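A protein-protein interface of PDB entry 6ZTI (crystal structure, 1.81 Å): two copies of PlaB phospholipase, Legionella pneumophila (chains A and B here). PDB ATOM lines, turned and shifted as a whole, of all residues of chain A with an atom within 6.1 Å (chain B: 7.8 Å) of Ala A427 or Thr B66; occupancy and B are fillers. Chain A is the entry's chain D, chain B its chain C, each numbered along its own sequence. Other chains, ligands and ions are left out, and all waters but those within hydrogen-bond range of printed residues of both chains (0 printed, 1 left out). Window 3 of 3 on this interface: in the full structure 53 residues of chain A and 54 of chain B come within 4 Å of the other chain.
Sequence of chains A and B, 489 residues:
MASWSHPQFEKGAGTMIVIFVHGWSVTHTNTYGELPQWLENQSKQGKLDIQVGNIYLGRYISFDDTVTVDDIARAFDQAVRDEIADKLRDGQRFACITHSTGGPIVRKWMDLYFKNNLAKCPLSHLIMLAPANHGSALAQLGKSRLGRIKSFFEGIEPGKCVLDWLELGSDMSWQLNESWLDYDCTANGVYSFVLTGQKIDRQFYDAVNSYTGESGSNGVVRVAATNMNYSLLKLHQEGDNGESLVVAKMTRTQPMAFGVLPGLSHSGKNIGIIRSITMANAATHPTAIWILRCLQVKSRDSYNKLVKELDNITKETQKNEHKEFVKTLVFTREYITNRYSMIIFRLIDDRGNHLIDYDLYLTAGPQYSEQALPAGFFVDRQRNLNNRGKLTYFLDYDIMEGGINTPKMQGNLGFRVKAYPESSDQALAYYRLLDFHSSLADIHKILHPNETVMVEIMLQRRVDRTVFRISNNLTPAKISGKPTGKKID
The side-chain carboxylate (OD2) of Asp B71 is in salt-bridge range of the guanidinium group (NH2) of Arg A461, 2.6 Å away.
N of Leu A428 sits at hydrogen-bond distance from OD2 of Asp B64, 3.3 Å away.
O of Thr B66 sits at hydrogen-bond distance from NH2 of Arg A461, 2.7 Å away.
The backbone NH (N) of Thr B68 lies within hydrogen-bond range of the side-chain carboxylate (OD2) of Asp B71, at 2.8 Å.
The side-chain carboxylate of Asp B64 lies within hydrogen-bond range of the side-chain hydroxyl of Thr B66, 2.7 Å away.
The backbone carbonyl oxygen (O) of Leu A428 sits at hydrogen-bond distance from the backbone NH (N) of Asp A464 (2.8 Å).
Among the printed residues, pairs that only touch across the chains: Ala A427 with Thr B66 (3.3 Å), Ala A429 with Thr B66 (3.7 Å), Ala A429 with Asp B71 (3.8 Å) and Arg A461 with Thr B68 (3.8 Å).
Of the printed residues of chain B, Ala A427 touches Thr B66.
Of the printed residues of chain B, Arg A461 touches Thr B66, Thr B68 and Asp B71.
Printed residues of chain A within 4 Å of Asp B64: Leu A428 (3.3 Å).
Lys B160 touches none of the printed residues of chain A.
The nearest printed residue of chain A that does not touch Thr B66 is Leu A428 (4.1 Å).
Of the 12 printed residues of chain A, 4 touch a printed residue of chain B.
Printed residues of chain A that touch a printed residue of chain B: Ala A427, Leu A428, Ala A429 and Arg A461.
Hydrophobic or aromatic side chains of chain A that line the printed part of chain B: Ala A427, Leu A428 and Ala A429.
Along chain A the printed residues that touch a printed residue of chain B span positions 427 to 461.
Along chain B the printed residues that touch a printed residue of chain A span positions 64 to 71.
Among the printed residues, 7 pairs touch across the chains.
Among the printed residues, Asp or Glu carboxylates within 4 Å of a Lys or Arg side-chain nitrogen of the other chain: Arg A461 with Asp B71 (2.6 Å).
No position is printed for both chains.
Of the 7 pairs that touch across the chains among the printed residues, none has its exchanged pair printed and touching as well.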
ATOM      1  N   PRO A 421      24.074  23.903   8.007  1.00  0.00           N
ATOM      2  CA  PRO A 421      24.758  22.695   7.507  1.00  0.00           C
ATOM      3  C   PRO A 421      25.547  22.943   6.226  1.00  0.00           C
ATOM      4  O   PRO A 421      25.178  23.832   5.452  1.00  0.00           O
ATOM      5  CB  PRO A 421      23.611  21.716   7.252  1.00  0.00           C
ATOM      6  CG  PRO A 421      22.424  22.555   7.081  1.00  0.00           C
ATOM      7  CD  PRO A 421      22.613  23.817   7.854  1.00  0.00           C
ATOM      8  N   SER A 423      26.614  20.426   3.826  1.00  0.00           N
ATOM      9  CA  SER A 423      26.494  19.518   2.693  1.00  0.00           C
ATOM     10  C   SER A 423      25.127  18.854   2.687  1.00  0.00           C
ATOM     11  O   SER A 423      24.412  18.837   3.694  1.00  0.00           O
ATOM     12  CB  SER A 423      27.585  18.446   2.716  1.00  0.00           C
ATOM     13  OG  SER A 423      27.301  17.455   3.692  1.00  0.00           O
ATOM     14  N   SER A 424      24.784  18.282   1.526  1.00  0.00           N
ATOM     15  CA  SER A 424      23.537  17.531   1.400  1.00  0.00           C
ATOM     16  C   SER A 424      23.479  16.393   2.412  1.00  0.00           C
ATOM     17  O   SER A 424      22.424  16.122   2.996  1.00  0.00           O
ATOM     18  CB  SER A 424      23.389  16.988  -0.028  1.00  0.00           C
ATOM     19  OG  SER A 424      24.279  15.909  -0.271  1.00  0.00           O
ATOM     20  N   ASP A 425      24.612  15.724   2.645  1.00  0.00           N
ATOM     21  CA  ASP A 425      24.623  14.549   3.510  1.00  0.00           C
ATOM     22  C   ASP A 425      24.279  14.886   4.958  1.00  0.00           C
ATOM     23  O   ASP A 425      23.874  13.991   5.708  1.00  0.00           O
ATOM     24  CB  ASP A 425      25.991  13.870   3.444  1.00  0.00           C
ATOM     25  CG  ASP A 425      26.497  13.727   2.020  1.00  0.00           C
ATOM     26  OD1 ASP A 425      27.030  14.720   1.474  1.00  0.00           O
ATOM     27  OD2 ASP A 425      26.347  12.628   1.442  1.00  0.00           O
ATOM     28  N   GLN A 426      24.430  16.147   5.365  1.00  0.00           N
ATOM     29  CA  GLN A 426      24.052  16.573   6.709  1.00  0.00           C
ATOM     30  C   GLN A 426      22.629  17.117   6.766  1.00  0.00           C
ATOM     31  O   GLN A 426      21.925  16.909   7.760  1.00  0.00           O
ATOM     32  CB  GLN A 426      25.023  17.645   7.210  1.00  0.00           C
ATOM     33  CG  GLN A 426      26.485  17.237   7.156  1.00  0.00           C
ATOM     34  CD  GLN A 426      27.424  18.402   7.418  1.00  0.00           C
ATOM     35  OE1 GLN A 426      26.991  19.494   7.811  1.00  0.00           O
ATOM     36  NE2 GLN A 426      28.717  18.179   7.194  1.00  0.00           N
ATOM     37  N   ALA A 427      22.202  17.830   5.728  1.00  0.00           N
ATOM     38  CA  ALA A 427      20.846  18.351   5.649  1.00  0.00           C
ATOM     39  C   ALA A 427      20.508  18.574   4.186  1.00  0.00           C
ATOM     40  O   ALA A 427      21.396  18.740   3.347  1.00  0.00           O
ATOM     41  CB  ALA A 427      20.695  19.655   6.433  1.00  0.00           C
ATOM     42  N   LEU A 428      19.209  18.584   3.888  1.00  0.00           N
ATOM     43  CA  LEU A 428      18.774  18.826   2.521  1.00  0.00           C
ATOM     44  C   LEU A 428      18.755  20.308   2.171  1.00  0.00           C
ATOM     45  O   LEU A 428      18.649  20.644   0.989  1.00  0.00           O
ATOM     46  CB  LEU A 428      17.394  18.196   2.308  1.00  0.00           C
ATOM     47  CG  LEU A 428      17.439  16.664   2.419  1.00  0.00           C
ATOM     48  CD1 LEU A 428      16.051  16.079   2.360  1.00  0.00           C
ATOM     49  CD2 LEU A 428      18.304  16.052   1.342  1.00  0.00           C
ATOM     50  N   ALA A 429      18.815  21.195   3.163  1.00  0.00           N
ATOM     51  CA  ALA A 429      19.109  22.607   2.955  1.00  0.00           C
ATOM     52  C   ALA A 429      20.476  22.887   3.565  1.00  0.00           C
ATOM     53  O   ALA A 429      20.726  22.510   4.713  1.00  0.00           O
ATOM     54  CB  ALA A 429      18.040  23.498   3.590  1.00  0.00           C
ATOM     55  N   TYR A 430      21.359  23.539   2.812  1.00  0.00           N
ATOM     56  CA  TYR A 430      22.742  23.673   3.260  1.00  0.00           C
ATOM     57  C   TYR A 430      23.405  24.848   2.543  1.00  0.00           C
ATOM     58  O   TYR A 430      22.819  25.481   1.661  1.00  0.00           O
ATOM     59  CB  TYR A 430      23.512  22.364   3.027  1.00  0.00           C
ATOM     60  CG  TYR A 430      23.598  21.991   1.584  1.00  0.00           C
ATOM     61  CD1 TYR A 430      22.529  21.387   0.941  1.00  0.00           C
ATOM     62  CD2 TYR A 430      24.733  22.266   0.851  1.00  0.00           C
ATOM     63  CE1 TYR A 430      22.603  21.053  -0.399  1.00  0.00           C
ATOM     64  CE2 TYR A 430      24.813  21.945  -0.479  1.00  0.00           C
ATOM     65  CZ  TYR A 430      23.748  21.336  -1.101  1.00  0.00           C
ATOM     66  OH  TYR A 430      23.834  21.015  -2.437  1.00  0.00           O
ATOM     67  N   ARG A 461      21.381  29.845  -0.248  1.00  0.00           N
ATOM     68  CA  ARG A 461      20.750  28.714   0.418  1.00  0.00           C
ATOM     69  C   ARG A 461      20.488  27.645  -0.635  1.00  0.00           C
ATOM     70  O   ARG A 461      19.672  27.839  -1.544  1.00  0.00           O
ATOM     71  CB  ARG A 461      19.464  29.149   1.111  1.00  0.00           C
ATOM     72  CG  ARG A 461      18.817  28.030   1.915  1.00  0.00           C
ATOM     73  CD  ARG A 461      17.584  28.489   2.658  1.00  0.00           C
ATOM     74  NE  ARG A 461      16.922  27.367   3.330  1.00  0.00           N
ATOM     75  CZ  ARG A 461      17.242  26.916   4.543  1.00  0.00           C
ATOM     76  NH1 ARG A 461      18.215  27.490   5.242  1.00  0.00           N
ATOM     77  NH2 ARG A 461      16.581  25.887   5.064  1.00  0.00           N
ATOM     78  N   ASP A 464      18.404  20.679  -1.769  1.00  0.00           N
ATOM     79  CA  ASP A 464      18.492  19.478  -2.590  1.00  0.00           C
ATOM     80  C   ASP A 464      17.136  19.147  -3.205  1.00  0.00           C
ATOM     81  O   ASP A 464      16.077  19.330  -2.590  1.00  0.00           O
ATOM     82  CB  ASP A 464      19.009  18.311  -1.756  1.00  0.00           C
ATOM     83  CG  ASP A 464      19.408  17.102  -2.611  1.00  0.00           C
ATOM     84  OD1 ASP A 464      18.500  16.371  -3.032  1.00  0.00           O
ATOM     85  OD2 ASP A 464      20.618  16.881  -2.865  1.00  0.00           O
ATOM     86  N   PRO A 483      19.816  12.451  -0.517  1.00  0.00           N
ATOM     87  CA  PRO A 483      20.017  13.564  -1.451  1.00  0.00           C
ATOM     88  C   PRO A 483      20.261  13.072  -2.868  1.00  0.00           C
ATOM     89  O   PRO A 483      20.836  12.005  -3.089  1.00  0.00           O
ATOM     90  CB  PRO A 483      21.258  14.282  -0.900  1.00  0.00           C
ATOM     91  CG  PRO A 483      21.420  13.796   0.487  1.00  0.00           C
ATOM     92  CD  PRO A 483      20.854  12.417   0.524  1.00  0.00           C
ATOM     93  N   PHE B  63      10.403  15.827   7.684  1.00  0.00           N
ATOM     94  CA  PHE B  63      11.078  15.354   8.884  1.00  0.00           C
ATOM     95  C   PHE B  63      12.538  15.795   8.933  1.00  0.00           C
ATOM     96  O   PHE B  63      13.387  15.091   9.484  1.00  0.00           O
ATOM     97  CB  PHE B  63      10.976  13.831   8.984  1.00  0.00           C
ATOM     98  CG  PHE B  63      11.273  13.105   7.698  1.00  0.00           C
ATOM     99  CD1 PHE B  63      10.266  12.859   6.778  1.00  0.00           C
ATOM    100  CD2 PHE B  63      12.551  12.648   7.425  1.00  0.00           C
ATOM    101  CE1 PHE B  63      10.532  12.175   5.591  1.00  0.00           C
ATOM    102  CE2 PHE B  63      12.826  11.970   6.246  1.00  0.00           C
ATOM    103  CZ  PHE B  63      11.811  11.727   5.329  1.00  0.00           C
ATOM    104  N   ASP B  64      12.843  16.961   8.372  1.00  0.00           N
ATOM    105  CA  ASP B  64      14.193  17.507   8.368  1.00  0.00           C
ATOM    106  C   ASP B  64      14.143  18.877   9.024  1.00  0.00           C
ATOM    107  O   ASP B  64      13.473  19.785   8.521  1.00  0.00           O
ATOM    108  CB  ASP B  64      14.745  17.603   6.945  1.00  0.00           C
ATOM    109  CG  ASP B  64      16.207  18.033   6.908  1.00  0.00           C
ATOM    110  OD1 ASP B  64      16.598  18.927   7.691  1.00  0.00           O
ATOM    111  OD2 ASP B  64      16.965  17.475   6.086  1.00  0.00           O
ATOM    112  N   ASP B  65      14.858  19.027  10.139  1.00  0.00           N
ATOM    113  CA  ASP B  65      14.749  20.246  10.934  1.00  0.00           C
ATOM    114  C   ASP B  65      15.250  21.481  10.201  1.00  0.00           C
ATOM    115  O   ASP B  65      14.881  22.596  10.582  1.00  0.00           O
ATOM    116  CB  ASP B  65      15.511  20.094  12.250  1.00  0.00           C
ATOM    117  CG  ASP B  65      14.697  19.377  13.320  1.00  0.00           C
ATOM    118  OD1 ASP B  65      13.444  19.422  13.267  1.00  0.00           O
ATOM    119  OD2 ASP B  65      15.317  18.773  14.223  1.00  0.00           O
ATOM    120  N   THR B  66      16.056  21.316   9.151  1.00  0.00           N
ATOM    121  CA  THR B  66      16.585  22.460   8.422  1.00  0.00           C
ATOM    122  C   THR B  66      15.652  22.945   7.319  1.00  0.00           C
ATOM    123  O   THR B  66      15.802  24.082   6.858  1.00  0.00           O
ATOM    124  CB  THR B  66      17.946  22.116   7.811  1.00  0.00           C
ATOM    125  OG1 THR B  66      17.771  21.198   6.722  1.00  0.00           O
ATOM    126  CG2 THR B  66      18.865  21.487   8.864  1.00  0.00           C
ATOM    127  N   VAL B  67      14.685  22.136   6.908  1.00  0.00           N
ATOM    128  CA  VAL B  67      13.865  22.451   5.742  1.00  0.00           C
ATOM    129  C   VAL B  67      12.721  23.370   6.157  1.00  0.00           C
ATOM    130  O   VAL B  67      12.037  23.123   7.154  1.00  0.00           O
ATOM    131  CB  VAL B  67      13.355  21.162   5.078  1.00  0.00           C
ATOM    132  CG1 VAL B  67      12.287  21.458   4.030  1.00  0.00           C
ATOM    133  CG2 VAL B  67      14.538  20.398   4.452  1.00  0.00           C
ATOM    134  N   THR B  68      12.530  24.448   5.403  1.00  0.00           N
ATOM    135  CA  THR B  68      11.453  25.394   5.644  1.00  0.00           C
ATOM    136  C   THR B  68      10.326  25.218   4.621  1.00  0.00           C
ATOM    137  O   THR B  68      10.449  24.506   3.617  1.00  0.00           O
ATOM    138  CB  THR B  68      12.001  26.820   5.605  1.00  0.00           C
ATOM    139  OG1 THR B  68      12.372  27.137   4.263  1.00  0.00           O
ATOM    140  CG2 THR B  68      13.238  26.947   6.512  1.00  0.00           C
ATOM    141  N   VAL B  69       9.202  25.885   4.894  1.00  0.00           N
ATOM    142  CA  VAL B  69       8.077  25.829   3.968  1.00  0.00           C
ATOM    143  C   VAL B  69       8.442  26.542   2.675  1.00  0.00           C
ATOM    144  O   VAL B  69       8.051  26.119   1.582  1.00  0.00           O
ATOM    145  CB  VAL B  69       6.818  26.424   4.622  1.00  0.00           C
ATOM    146  CG1 VAL B  69       5.741  26.671   3.574  1.00  0.00           C
ATOM    147  CG2 VAL B  69       6.298  25.496   5.714  1.00  0.00           C
ATOM    148  N   ASP B  71      11.474  26.502   1.478  1.00  0.00           N
ATOM    149  CA  ASP B  71      12.260  25.469   0.802  1.00  0.00           C
ATOM    150  C   ASP B  71      11.363  24.501   0.043  1.00  0.00           C
ATOM    151  O   ASP B  71      11.615  24.186  -1.125  1.00  0.00           O
ATOM    152  CB  ASP B  71      13.093  24.663   1.809  1.00  0.00           C
ATOM    153  CG  ASP B  71      14.151  25.482   2.536  1.00  0.00           C
ATOM    154  OD1 ASP B  71      14.569  26.559   2.053  1.00  0.00           O
ATOM    155  OD2 ASP B  71      14.587  25.004   3.606  1.00  0.00           O
ATOM    156  N   GLY B 159       9.567  18.322  11.552  1.00  0.00           N
ATOM    157  CA  GLY B 159      10.694  19.226  11.427  1.00  0.00           C
ATOM    158  C   GLY B 159      10.422  20.574  12.082  1.00  0.00           C
ATOM    159  O   GLY B 159       9.361  21.169  11.907  1.00  0.00           O
ATOM    160  N   LYS B 160      11.420  21.064  12.811  1.00  0.00           N
ATOM    161  CA  LYS B 160      11.198  22.231  13.655  1.00  0.00           C
ATOM    162  C   LYS B 160      10.752  23.435  12.837  1.00  0.00           C
ATOM    163  O   LYS B 160       9.826  24.155  13.234  1.00  0.00           O
ATOM    164  CB  LYS B 160      12.468  22.548  14.444  1.00  0.00           C
ATOM    165  CG  LYS B 160      12.239  23.515  15.606  1.00  0.00           C
ATOM    166  CD  LYS B 160      12.464  24.967  15.195  1.00  0.00           C
ATOM    167  CE  LYS B 160      12.140  25.925  16.330  1.00  0.00           C
ATOM    168  NZ  LYS B 160      12.344  27.342  15.924  1.00  0.00           N
ATOM    169  N   CYS B 161      11.371  23.660  11.675  1.00  0.00           N
ATOM    170  CA  CYS B 161      11.018  24.848  10.902  1.00  0.00           C
ATOM    171  C   CYS B 161       9.601  24.785  10.358  1.00  0.00           C
ATOM    172  O   CYS B 161       8.966  25.828  10.185  1.00  0.00           O
ATOM    173  CB  CYS B 161      12.002  25.055   9.761  1.00  0.00           C
ATOM    174  SG  CYS B 161      13.612  25.509  10.378  1.00  0.00           S
ATOM    175  N   VAL B 162       9.097  23.594  10.044  1.00  0.00           N
ATOM    176  CA  VAL B 162       7.706  23.512   9.618  1.00  0.00           C
ATOM    177  C   VAL B 162       6.763  23.738  10.804  1.00  0.00           C
ATOM    178  O   VAL B 162       5.679  24.314  10.646  1.00  0.00           O
ATOM    179  CB  VAL B 162       7.443  22.159   8.932  1.00  0.00           C
ATOM    180  CG1 VAL B 162       5.950  21.980   8.652  1.00  0.00           C
ATOM    181  CG2 VAL B 162       8.228  22.066   7.643  1.00  0.00           C
